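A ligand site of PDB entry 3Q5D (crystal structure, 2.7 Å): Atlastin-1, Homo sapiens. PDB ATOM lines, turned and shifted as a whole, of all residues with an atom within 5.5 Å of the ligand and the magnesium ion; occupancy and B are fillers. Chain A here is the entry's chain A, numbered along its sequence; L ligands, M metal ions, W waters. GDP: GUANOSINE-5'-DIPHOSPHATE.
O3B of the ligand is in hydrogen-bond range of N of Arg 77, at 2.9 Å. O of Val 276 lies within hydrogen-bond range of O2' of the ligand. The backbone carbonyl oxygen (O) of Asn 279 is in hydrogen-bond range of an oxygen (O3') of the ligand (2.7 Å). O1B of the ligand lies within salt-bridge range of NZ of Lys 80 (2.6 Å). The backbone NH (N) of Gly 79 is in hydrogen-bond range of an oxygen (O1B) of the ligand, at 3.1 Å. O2A of the ligand lies within hydrogen-bond range of N of Phe 82, at 3.0 Å. The guanidinium group (NH2) of Arg 217 is in hydrogen-bond range of an oxygen (O6) of the ligand, 2.6 Å away. An oxygen (O1B) of the ligand lies within hydrogen-bond range of the backbone NH (N) of Lys 80, 3.0 Å away. The backbone NH (N) of Lys 78 lies within hydrogen-bond range of an oxygen (O1B) of the ligand (2.9 Å). O2A of the ligand is in hydrogen-bond range of N of Ser 81, 3.1 Å away. N1 of the ligand lies within hydrogen-bond range of OD1 of Asp 218, at 2.7 Å.
O of Asn 281 sits close to ND2 of Asn 279, at 3.4 Å. NZ of Lys 80 sits at hydrogen-bond distance from OE1 of Gln 148. N of Phe 282 lies close to ND2 of Asn 279. NZ of Lys 80 lies within hydrogen-bond range of O of Ala 75 (2.8 Å). NH1 of Arg 217 is in hydrogen-bond range of O of Gly 79 (2.9 Å).
O of Ala 75 touches O1B of the ligand, at 3.9 Å. CD1 of Phe 76 touches O3B of the ligand (3.7 Å). Gln 148 touches the ligand. His 271 touches the ligand (NE2 to N2, 3.6 Å). Pro 272 touches the ligand (CD to N1, 3.2 Å). Ala 277 touches the ligand. Pro 280 touches the ligand. Phe 293 touches the ligand. Hydrophobic or aromatic side chains within 4 Å of the ligand: Phe 76, Phe 82, Pro 272, Val 276, Ala 277 and Phe 293. Of the 29 residues printed, 18 come within 4 Å of the ligand. The nearest printed residue that does not touch the ligand is Phe 282 (4.1 Å).
Glu 117 touches the magnesium ion (OE2 to MG, 3.4 Å). Gln 148 touches the magnesium ion (OE1 to MG, 3.9 Å). Of the 29 residues printed, 3 come within 4 Å of the magnesium ion.
The magnesium ion is bound by the side-chain hydroxyl of Ser 81 and an oxygen (O2B) of the ligand.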
ATOM      1  N   ALA A  75      -3.690   2.700  37.824  1.00  0.00           N
ATOM      2  CA  ALA A  75      -2.374   2.548  37.195  1.00  0.00           C
ATOM      3  C   ALA A  75      -2.496   2.294  35.693  1.00  0.00           C
ATOM      4  O   ALA A  75      -3.580   2.077  35.154  1.00  0.00           O
ATOM      5  CB  ALA A  75      -1.601   1.433  37.875  1.00  0.00           C
ATOM      6  N   PHE A  76      -1.342   2.361  35.035  1.00  0.00           N
ATOM      7  CA  PHE A  76      -1.157   2.118  33.610  1.00  0.00           C
ATOM      8  C   PHE A  76      -1.308   0.622  33.290  1.00  0.00           C
ATOM      9  O   PHE A  76      -0.877  -0.236  34.077  1.00  0.00           O
ATOM     10  CB  PHE A  76       0.245   2.641  33.235  1.00  0.00           C
ATOM     11  CG  PHE A  76       0.647   2.431  31.808  1.00  0.00           C
ATOM     12  CD1 PHE A  76       0.048   3.143  30.772  1.00  0.00           C
ATOM     13  CD2 PHE A  76       1.710   1.571  31.490  1.00  0.00           C
ATOM     14  CE1 PHE A  76       0.446   2.963  29.457  1.00  0.00           C
ATOM     15  CE2 PHE A  76       2.121   1.397  30.176  1.00  0.00           C
ATOM     16  CZ  PHE A  76       1.489   2.093  29.159  1.00  0.00           C
ATOM     17  N   ARG A  77      -1.934   0.322  32.158  1.00  0.00           N
ATOM     18  CA  ARG A  77      -2.143  -1.059  31.720  1.00  0.00           C
ATOM     19  C   ARG A  77      -3.027  -1.827  32.682  1.00  0.00           C
ATOM     20  O   ARG A  77      -2.728  -2.976  33.012  1.00  0.00           O
ATOM     21  CB  ARG A  77      -0.810  -1.799  31.572  1.00  0.00           C
ATOM     22  CG  ARG A  77      -0.011  -1.323  30.409  1.00  0.00           C
ATOM     23  CD  ARG A  77       0.761  -2.454  29.827  1.00  0.00           C
ATOM     24  NE  ARG A  77       1.503  -2.038  28.645  1.00  0.00           N
ATOM     25  CZ  ARG A  77       2.831  -1.976  28.575  1.00  0.00           C
ATOM     26  NH1 ARG A  77       3.561  -2.315  29.632  1.00  0.00           N
ATOM     27  NH2 ARG A  77       3.410  -1.603  27.450  1.00  0.00           N
ATOM     28  N   LYS A  78      -4.078  -1.178  33.150  1.00  0.00           N
ATOM     29  CA  LYS A  78      -5.064  -1.839  34.006  1.00  0.00           C
ATOM     30  C   LYS A  78      -6.401  -1.994  33.251  1.00  0.00           C
ATOM     31  O   LYS A  78      -7.400  -2.406  33.821  1.00  0.00           O
ATOM     32  CB  LYS A  78      -5.220  -1.057  35.306  1.00  0.00           C
ATOM     33  CG  LYS A  78      -4.434  -1.614  36.483  1.00  0.00           C
ATOM     34  CD  LYS A  78      -3.016  -1.912  36.097  1.00  0.00           C
ATOM     35  CE  LYS A  78      -2.471  -3.089  36.899  1.00  0.00           C
ATOM     36  NZ  LYS A  78      -2.262  -2.739  38.322  1.00  0.00           N
ATOM     37  N   GLY A  79      -6.380  -1.662  31.957  1.00  0.00           N
ATOM     38  CA  GLY A  79      -7.531  -1.858  31.097  1.00  0.00           C
ATOM     39  C   GLY A  79      -8.522  -0.706  31.070  1.00  0.00           C
ATOM     40  O   GLY A  79      -9.697  -0.903  30.737  1.00  0.00           O
ATOM     41  N   LYS A  80      -8.072   0.488  31.422  1.00  0.00           N
ATOM     42  CA  LYS A  80      -8.972   1.627  31.511  1.00  0.00           C
ATOM     43  C   LYS A  80      -9.497   2.035  30.152  1.00  0.00           C
ATOM     44  O   LYS A  80     -10.687   2.324  30.015  1.00  0.00           O
ATOM     45  CB  LYS A  80      -8.318   2.832  32.214  1.00  0.00           C
ATOM     46  CG  LYS A  80      -7.944   2.597  33.686  1.00  0.00           C
ATOM     47  CD  LYS A  80      -7.281   3.852  34.278  1.00  0.00           C
ATOM     48  CE  LYS A  80      -6.125   4.376  33.377  1.00  0.00           C
ATOM     49  NZ  LYS A  80      -5.018   3.391  33.098  1.00  0.00           N
ATOM     50  N   SER A  81      -8.627   2.061  29.129  1.00  0.00           N
ATOM     51  CA  SER A  81      -9.046   2.622  27.855  1.00  0.00           C
ATOM     52  C   SER A  81     -10.034   1.703  27.171  1.00  0.00           C
ATOM     53  O   SER A  81     -10.969   2.155  26.514  1.00  0.00           O
ATOM     54  CB  SER A  81      -7.851   2.912  26.947  1.00  0.00           C
ATOM     55  OG  SER A  81      -7.136   4.028  27.420  1.00  0.00           O
ATOM     56  N   PHE A  82      -9.811   0.411  27.351  1.00  0.00           N
ATOM     57  CA  PHE A  82     -10.699  -0.601  26.834  1.00  0.00           C
ATOM     58  C   PHE A  82     -12.060  -0.417  27.460  1.00  0.00           C
ATOM     59  O   PHE A  82     -13.088  -0.494  26.788  1.00  0.00           O
ATOM     60  CB  PHE A  82     -10.147  -1.963  27.196  1.00  0.00           C
ATOM     61  CG  PHE A  82     -10.753  -3.078  26.438  1.00  0.00           C
ATOM     62  CD1 PHE A  82     -10.553  -3.203  25.083  1.00  0.00           C
ATOM     63  CD2 PHE A  82     -11.492  -4.047  27.091  1.00  0.00           C
ATOM     64  CE1 PHE A  82     -11.097  -4.272  24.380  1.00  0.00           C
ATOM     65  CE2 PHE A  82     -12.025  -5.123  26.394  1.00  0.00           C
ATOM     66  CZ  PHE A  82     -11.842  -5.229  25.038  1.00  0.00           C
ATOM     67  N   LEU A  83     -12.093  -0.187  28.774  1.00  0.00           N
ATOM     68  CA  LEU A  83     -13.388  -0.016  29.419  1.00  0.00           C
ATOM     69  C   LEU A  83     -14.040   1.247  28.885  1.00  0.00           C
ATOM     70  O   LEU A  83     -15.190   1.220  28.434  1.00  0.00           O
ATOM     71  CB  LEU A  83     -13.252   0.043  30.935  1.00  0.00           C
ATOM     72  CG  LEU A  83     -14.544   0.503  31.636  1.00  0.00           C
ATOM     73  CD1 LEU A  83     -15.595  -0.592  31.595  1.00  0.00           C
ATOM     74  CD2 LEU A  83     -14.249   0.937  33.073  1.00  0.00           C
ATOM     75  N   TRP A 112     -10.056   5.771  22.984  1.00  0.00           N
ATOM     76  CA  TRP A 112      -9.085   6.379  23.876  1.00  0.00           C
ATOM     77  C   TRP A 112      -7.718   5.789  23.625  1.00  0.00           C
ATOM     78  O   TRP A 112      -6.703   6.366  24.019  1.00  0.00           O
ATOM     79  CB  TRP A 112      -9.449   6.071  25.320  1.00  0.00           C
ATOM     80  CG  TRP A 112     -10.691   6.674  25.824  1.00  0.00           C
ATOM     81  CD1 TRP A 112     -11.958   6.202  25.658  1.00  0.00           C
ATOM     82  CD2 TRP A 112     -10.793   7.847  26.628  1.00  0.00           C
ATOM     83  NE1 TRP A 112     -12.851   7.015  26.307  1.00  0.00           N
ATOM     84  CE2 TRP A 112     -12.166   8.038  26.908  1.00  0.00           C
ATOM     85  CE3 TRP A 112      -9.873   8.773  27.126  1.00  0.00           C
ATOM     86  CZ2 TRP A 112     -12.630   9.112  27.659  1.00  0.00           C
ATOM     87  CZ3 TRP A 112     -10.331   9.831  27.880  1.00  0.00           C
ATOM     88  CH2 TRP A 112     -11.707   9.996  28.139  1.00  0.00           C
ATOM     89  N   ARG A 113      -7.705   4.619  22.976  1.00  0.00           N
ATOM     90  CA  ARG A 113      -6.474   3.886  22.680  1.00  0.00           C
ATOM     91  C   ARG A 113      -5.710   4.502  21.493  1.00  0.00           C
ATOM     92  O   ARG A 113      -6.169   4.460  20.340  1.00  0.00           O
ATOM     93  CB  ARG A 113      -6.771   2.394  22.457  1.00  0.00           C
ATOM     94  CG  ARG A 113      -7.423   1.693  23.681  1.00  0.00           C
ATOM     95  CD  ARG A 113      -7.850   0.240  23.413  1.00  0.00           C
ATOM     96  NE  ARG A 113      -9.086   0.158  22.622  1.00  0.00           N
ATOM     97  CZ  ARG A 113      -9.529  -0.940  22.004  1.00  0.00           C
ATOM     98  NH1 ARG A 113      -8.834  -2.076  22.084  1.00  0.00           N
ATOM     99  NH2 ARG A 113     -10.655  -0.897  21.307  1.00  0.00           N
ATOM    100  N   GLU A 117       1.663   4.000  23.094  1.00  0.00           N
ATOM    101  CA  GLU A 117       1.177   4.363  24.421  1.00  0.00           C
ATOM    102  C   GLU A 117       2.330   4.647  25.384  1.00  0.00           C
ATOM    103  O   GLU A 117       3.098   3.749  25.731  1.00  0.00           O
ATOM    104  CB  GLU A 117       0.276   3.259  25.004  1.00  0.00           C
ATOM    105  CG  GLU A 117      -0.796   3.744  25.972  1.00  0.00           C
ATOM    106  CD  GLU A 117      -2.159   3.990  25.313  1.00  0.00           C
ATOM    107  OE1 GLU A 117      -2.379   3.462  24.199  1.00  0.00           O
ATOM    108  OE2 GLU A 117      -3.005   4.702  25.903  1.00  0.00           O
ATOM    109  N   GLN A 124      -6.868  12.904  31.261  1.00  0.00           N
ATOM    110  CA  GLN A 124      -7.348  13.153  29.906  1.00  0.00           C
ATOM    111  C   GLN A 124      -8.867  13.279  30.002  1.00  0.00           C
ATOM    112  O   GLN A 124      -9.512  12.524  30.744  1.00  0.00           O
ATOM    113  CB  GLN A 124      -6.974  11.997  28.956  1.00  0.00           C
ATOM    114  CG  GLN A 124      -5.485  11.851  28.605  1.00  0.00           C
ATOM    115  CD  GLN A 124      -5.171  10.583  27.779  1.00  0.00           C
ATOM    116  OE1 GLN A 124      -5.926   9.600  27.772  1.00  0.00           O
ATOM    117  NE2 GLN A 124      -4.028  10.607  27.093  1.00  0.00           N
ATOM    118  N   ASP A 146     -10.025  10.223  31.931  1.00  0.00           N
ATOM    119  CA  ASP A 146      -9.122   9.152  32.308  1.00  0.00           C
ATOM    120  C   ASP A 146      -8.127   9.706  33.317  1.00  0.00           C
ATOM    121  O   ASP A 146      -7.499  10.733  33.074  1.00  0.00           O
ATOM    122  CB  ASP A 146      -8.385   8.639  31.094  1.00  0.00           C
ATOM    123  CG  ASP A 146      -7.426   7.532  31.439  1.00  0.00           C
ATOM    124  OD1 ASP A 146      -7.702   6.366  31.088  1.00  0.00           O
ATOM    125  OD2 ASP A 146      -6.385   7.836  32.075  1.00  0.00           O
ATOM    126  N   GLN A 148      -4.789   8.775  35.413  1.00  0.00           N
ATOM    127  CA  GLN A 148      -3.739   7.778  35.388  1.00  0.00           C
ATOM    128  C   GLN A 148      -2.484   8.177  36.137  1.00  0.00           C
ATOM    129  O   GLN A 148      -2.014   9.312  36.068  1.00  0.00           O
ATOM    130  CB  GLN A 148      -3.403   7.421  33.940  1.00  0.00           C
ATOM    131  CG  GLN A 148      -2.355   6.339  33.803  1.00  0.00           C
ATOM    132  CD  GLN A 148      -2.181   5.873  32.373  1.00  0.00           C
ATOM    133  OE1 GLN A 148      -2.938   5.033  31.890  1.00  0.00           O
ATOM    134  NE2 GLN A 148      -1.161   6.414  31.680  1.00  0.00           N
ATOM    135  N   ARG A 217     -10.977  -5.549  38.312  1.00  0.00           N
ATOM    136  CA  ARG A 217     -10.905  -5.907  36.896  1.00  0.00           C
ATOM    137  C   ARG A 217     -10.769  -7.351  36.443  1.00  0.00           C
ATOM    138  O   ARG A 217     -11.241  -7.674  35.348  1.00  0.00           O
ATOM    139  CB  ARG A 217      -9.873  -5.066  36.154  1.00  0.00           C
ATOM    140  CG  ARG A 217     -10.335  -3.655  35.867  1.00  0.00           C
ATOM    141  CD  ARG A 217     -11.672  -3.657  35.165  1.00  0.00           C
ATOM    142  NE  ARG A 217     -11.520  -4.096  33.781  1.00  0.00           N
ATOM    143  CZ  ARG A 217     -11.184  -3.272  32.811  1.00  0.00           C
ATOM    144  NH1 ARG A 217     -10.971  -1.986  33.099  1.00  0.00           N
ATOM    145  NH2 ARG A 217     -11.058  -3.725  31.555  1.00  0.00           N
ATOM    146  N   ASP A 218     -10.134  -8.231  37.207  1.00  0.00           N
ATOM    147  CA  ASP A 218     -10.027  -9.590  36.619  1.00  0.00           C
ATOM    148  C   ASP A 218     -10.470 -10.652  37.611  1.00  0.00           C
ATOM    149  O   ASP A 218      -9.768 -11.629  37.844  1.00  0.00           O
ATOM    150  CB  ASP A 218      -8.596  -9.904  36.137  1.00  0.00           C
ATOM    151  CG  ASP A 218      -8.275  -9.391  34.720  1.00  0.00           C
ATOM    152  OD1 ASP A 218      -9.197  -9.042  33.953  1.00  0.00           O
ATOM    153  OD2 ASP A 218      -7.069  -9.384  34.380  1.00  0.00           O
ATOM    154  N   LEU A 269     -15.766  -7.464  37.920  1.00  0.00           N
ATOM    155  CA  LEU A 269     -15.763  -7.711  36.471  1.00  0.00           C
ATOM    156  C   LEU A 269     -14.916  -8.934  36.081  1.00  0.00           C
ATOM    157  O   LEU A 269     -13.813  -9.109  36.572  1.00  0.00           O
ATOM    158  CB  LEU A 269     -15.305  -6.468  35.718  1.00  0.00           C
ATOM    159  CG  LEU A 269     -15.683  -6.401  34.240  1.00  0.00           C
ATOM    160  CD1 LEU A 269     -17.202  -6.397  34.077  1.00  0.00           C
ATOM    161  CD2 LEU A 269     -15.038  -5.156  33.574  1.00  0.00           C
ATOM    162  N   PRO A 270     -15.455  -9.815  35.238  1.00  0.00           N
ATOM    163  CA  PRO A 270     -14.636 -10.999  34.900  1.00  0.00           C
ATOM    164  C   PRO A 270     -13.483 -10.743  33.918  1.00  0.00           C
ATOM    165  O   PRO A 270     -13.332  -9.673  33.336  1.00  0.00           O
ATOM    166  CB  PRO A 270     -15.657 -11.979  34.293  1.00  0.00           C
ATOM    167  CG  PRO A 270     -16.843 -11.149  33.936  1.00  0.00           C
ATOM    168  CD  PRO A 270     -16.879 -10.032  34.937  1.00  0.00           C
ATOM    169  N   HIS A 271     -12.656 -11.760  33.770  1.00  0.00           N
ATOM    170  CA  HIS A 271     -11.490 -11.706  32.886  1.00  0.00           C
ATOM    171  C   HIS A 271     -12.005 -11.778  31.476  1.00  0.00           C
ATOM    172  O   HIS A 271     -12.847 -12.623  31.167  1.00  0.00           O
ATOM    173  CB  HIS A 271     -10.550 -12.885  33.169  1.00  0.00           C
ATOM    174  CG  HIS A 271      -9.213 -12.760  32.513  1.00  0.00           C
ATOM    175  ND1 HIS A 271      -9.027 -12.891  31.157  1.00  0.00           N
ATOM    176  CD2 HIS A 271      -7.980 -12.509  33.038  1.00  0.00           C
ATOM    177  CE1 HIS A 271      -7.745 -12.727  30.864  1.00  0.00           C
ATOM    178  NE2 HIS A 271      -7.092 -12.502  31.983  1.00  0.00           N
ATOM    179  N   PRO A 272     -11.512 -10.886  30.603  1.00  0.00           N
ATOM    180  CA  PRO A 272     -11.998 -10.744  29.236  1.00  0.00           C
ATOM    181  C   PRO A 272     -11.501 -11.809  28.267  1.00  0.00           C
ATOM    182  O   PRO A 272     -11.937 -11.815  27.115  1.00  0.00           O
ATOM    183  CB  PRO A 272     -11.461  -9.377  28.831  1.00  0.00           C
ATOM    184  CG  PRO A 272     -10.228  -9.238  29.625  1.00  0.00           C
ATOM    185  CD  PRO A 272     -10.536  -9.837  30.950  1.00  0.00           C
ATOM    186  N   VAL A 276      -7.976 -10.585  24.325  1.00  0.00           N
ATOM    187  CA  VAL A 276      -8.024  -9.179  24.750  1.00  0.00           C
ATOM    188  C   VAL A 276      -6.796  -8.896  25.627  1.00  0.00           C
ATOM    189  O   VAL A 276      -6.192  -7.821  25.561  1.00  0.00           O
ATOM    190  CB  VAL A 276      -9.316  -8.854  25.536  1.00  0.00           C
ATOM    191  CG1 VAL A 276      -9.166  -7.617  26.434  1.00  0.00           C
ATOM    192  CG2 VAL A 276     -10.503  -8.706  24.596  1.00  0.00           C
ATOM    193  N   ALA A 277      -6.425  -9.900  26.414  1.00  0.00           N
ATOM    194  CA  ALA A 277      -5.487  -9.709  27.506  1.00  0.00           C
ATOM    195  C   ALA A 277      -4.036  -9.577  27.069  1.00  0.00           C
ATOM    196  O   ALA A 277      -3.295  -8.827  27.690  1.00  0.00           O
ATOM    197  CB  ALA A 277      -5.603 -10.829  28.489  1.00  0.00           C
ATOM    198  N   THR A 278      -3.654 -10.310  26.024  1.00  0.00           N
ATOM    199  CA  THR A 278      -2.257 -10.373  25.588  1.00  0.00           C
ATOM    200  C   THR A 278      -2.060  -9.659  24.271  1.00  0.00           C
ATOM    201  O   THR A 278      -0.983  -9.711  23.681  1.00  0.00           O
ATOM    202  CB  THR A 278      -1.756 -11.822  25.373  1.00  0.00           C
ATOM    203  OG1 THR A 278      -2.635 -12.517  24.487  1.00  0.00           O
ATOM    204  CG2 THR A 278      -1.687 -12.575  26.674  1.00  0.00           C
ATOM    205  N   ASN A 279      -3.103  -9.016  23.784  1.00  0.00           N
ATOM    206  CA  ASN A 279      -3.058  -8.283  22.527  1.00  0.00           C
ATOM    207  C   ASN A 279      -3.195  -6.819  22.867  1.00  0.00           C
ATOM    208  O   ASN A 279      -4.248  -6.396  23.327  1.00  0.00           O
ATOM    209  CB  ASN A 279      -4.211  -8.755  21.637  1.00  0.00           C
ATOM    210  CG  ASN A 279      -4.294  -8.016  20.299  1.00  0.00           C
ATOM    211  OD1 ASN A 279      -4.889  -8.519  19.339  1.00  0.00           O
ATOM    212  ND2 ASN A 279      -3.714  -6.816  20.233  1.00  0.00           N
ATOM    213  N   PRO A 280      -2.136  -6.030  22.668  1.00  0.00           N
ATOM    214  CA  PRO A 280      -2.249  -4.585  22.878  1.00  0.00           C
ATOM    215  C   PRO A 280      -3.061  -4.126  21.685  1.00  0.00           C
ATOM    216  O   PRO A 280      -2.987  -4.771  20.638  1.00  0.00           O
ATOM    217  CB  PRO A 280      -0.814  -4.118  22.737  1.00  0.00           C
ATOM    218  CG  PRO A 280      -0.309  -4.986  21.631  1.00  0.00           C
ATOM    219  CD  PRO A 280      -0.917  -6.363  21.898  1.00  0.00           C
ATOM    220  N   ASN A 281      -3.829  -3.062  21.791  1.00  0.00           N
ATOM    221  CA  ASN A 281      -4.728  -2.785  20.663  1.00  0.00           C
ATOM    222  C   ASN A 281      -5.553  -3.999  20.151  1.00  0.00           C
ATOM    223  O   ASN A 281      -5.535  -4.283  18.969  1.00  0.00           O
ATOM    224  CB  ASN A 281      -3.976  -2.145  19.487  1.00  0.00           C
ATOM    225  CG  ASN A 281      -4.921  -1.593  18.415  1.00  0.00           C
ATOM    226  OD1 ASN A 281      -4.598  -1.582  17.233  1.00  0.00           O
ATOM    227  ND2 ASN A 281      -6.101  -1.136  18.839  1.00  0.00           N
ATOM    228  N   PHE A 282      -6.296  -4.670  21.028  1.00  0.00           N
ATOM    229  CA  PHE A 282      -7.224  -5.747  20.609  1.00  0.00           C
ATOM    230  C   PHE A 282      -8.180  -5.274  19.516  1.00  0.00           C
ATOM    231  O   PHE A 282      -8.711  -4.163  19.591  1.00  0.00           O
ATOM    232  CB  PHE A 282      -8.018  -6.293  21.797  1.00  0.00           C
ATOM    233  CG  PHE A 282      -9.120  -7.221  21.396  1.00  0.00           C
ATOM    234  CD1 PHE A 282     -10.393  -6.742  21.152  1.00  0.00           C
ATOM    235  CD2 PHE A 282      -8.887  -8.573  21.233  1.00  0.00           C
ATOM    236  CE1 PHE A 282     -11.410  -7.579  20.747  1.00  0.00           C
ATOM    237  CE2 PHE A 282      -9.903  -9.418  20.846  1.00  0.00           C
ATOM    238  CZ  PHE A 282     -11.164  -8.929  20.594  1.00  0.00           C
ATOM    239  N   PHE A 293     -17.845 -11.683  30.270  1.00  0.00           N
ATOM    240  CA  PHE A 293     -17.299 -10.344  30.431  1.00  0.00           C
ATOM    241  C   PHE A 293     -18.190  -9.362  29.720  1.00  0.00           C
ATOM    242  O   PHE A 293     -18.569  -8.355  30.302  1.00  0.00           O
ATOM    243  CB  PHE A 293     -15.852 -10.263  29.919  1.00  0.00           C
ATOM    244  CG  PHE A 293     -15.302  -8.848  29.838  1.00  0.00           C
ATOM    245  CD1 PHE A 293     -14.501  -8.345  30.838  1.00  0.00           C
ATOM    246  CD2 PHE A 293     -15.564  -8.049  28.733  1.00  0.00           C
ATOM    247  CE1 PHE A 293     -14.003  -7.060  30.764  1.00  0.00           C
ATOM    248  CE2 PHE A 293     -15.058  -6.763  28.647  1.00  0.00           C
ATOM    249  CZ  PHE A 293     -14.274  -6.258  29.661  1.00  0.00           C
HETATM  250  PB  GDP L   1      -4.774   1.272  30.239  1.00  0.00           P
HETATM  251  O1B GDP L   1      -5.119   1.167  31.701  1.00  0.00           O
HETATM  252  O2B GDP L   1      -5.747   2.179  29.517  1.00  0.00           O
HETATM  253  O3B GDP L   1      -3.378   1.875  30.150  1.00  0.00           O
HETATM  254  O3A GDP L   1      -4.848  -0.195  29.595  1.00  0.00           O
HETATM  255  PA  GDP L   1      -5.466  -0.539  28.137  1.00  0.00           P
HETATM  256  O1A GDP L   1      -4.764   0.177  27.000  1.00  0.00           O
HETATM  257  O2A GDP L   1      -6.955  -0.283  28.098  1.00  0.00           O
HETATM  258  O5' GDP L   1      -5.230  -2.120  28.030  1.00  0.00           O
HETATM  259  C5' GDP L   1      -4.000  -2.734  28.407  1.00  0.00           C
HETATM  260  C4' GDP L   1      -3.980  -4.144  27.841  1.00  0.00           C
HETATM  261  O4' GDP L   1      -4.831  -5.014  28.604  1.00  0.00           O
HETATM  262  C3' GDP L   1      -4.526  -4.179  26.429  1.00  0.00           C
HETATM  263  O3' GDP L   1      -3.878  -5.263  25.771  1.00  0.00           O
HETATM  264  C2' GDP L   1      -5.988  -4.538  26.618  1.00  0.00           C
HETATM  265  O2' GDP L   1      -6.538  -5.170  25.457  1.00  0.00           O
HETATM  266  C1' GDP L   1      -5.934  -5.475  27.811  1.00  0.00           C
HETATM  267  N9  GDP L   1      -7.165  -5.384  28.632  1.00  0.00           N
HETATM  268  C8  GDP L   1      -8.151  -4.484  28.532  1.00  0.00           C
HETATM  269  N7  GDP L   1      -9.098  -4.712  29.479  1.00  0.00           N
HETATM  270  C5  GDP L   1      -8.711  -5.765  30.222  1.00  0.00           C
HETATM  271  C6  GDP L   1      -9.229  -6.533  31.380  1.00  0.00           C
HETATM  272  O6  GDP L   1     -10.317  -6.237  31.910  1.00  0.00           O
HETATM  273  N1  GDP L   1      -8.487  -7.564  31.837  1.00  0.00           N
HETATM  274  C2  GDP L   1      -7.306  -7.892  31.249  1.00  0.00           C
HETATM  275  N2  GDP L   1      -6.556  -8.922  31.694  1.00  0.00           N
HETATM  276  N3  GDP L   1      -6.799  -7.238  30.196  1.00  0.00           N
HETATM  277  C4  GDP L   1      -7.432  -6.196  29.643  1.00  0.00           C
HETATM  278 MG    MG M   1      -5.034   4.436  28.648  1.00  0.00          MG
HETATM  279  O   HOH W   1      -6.656  -3.385  23.604  1.00  0.00           O
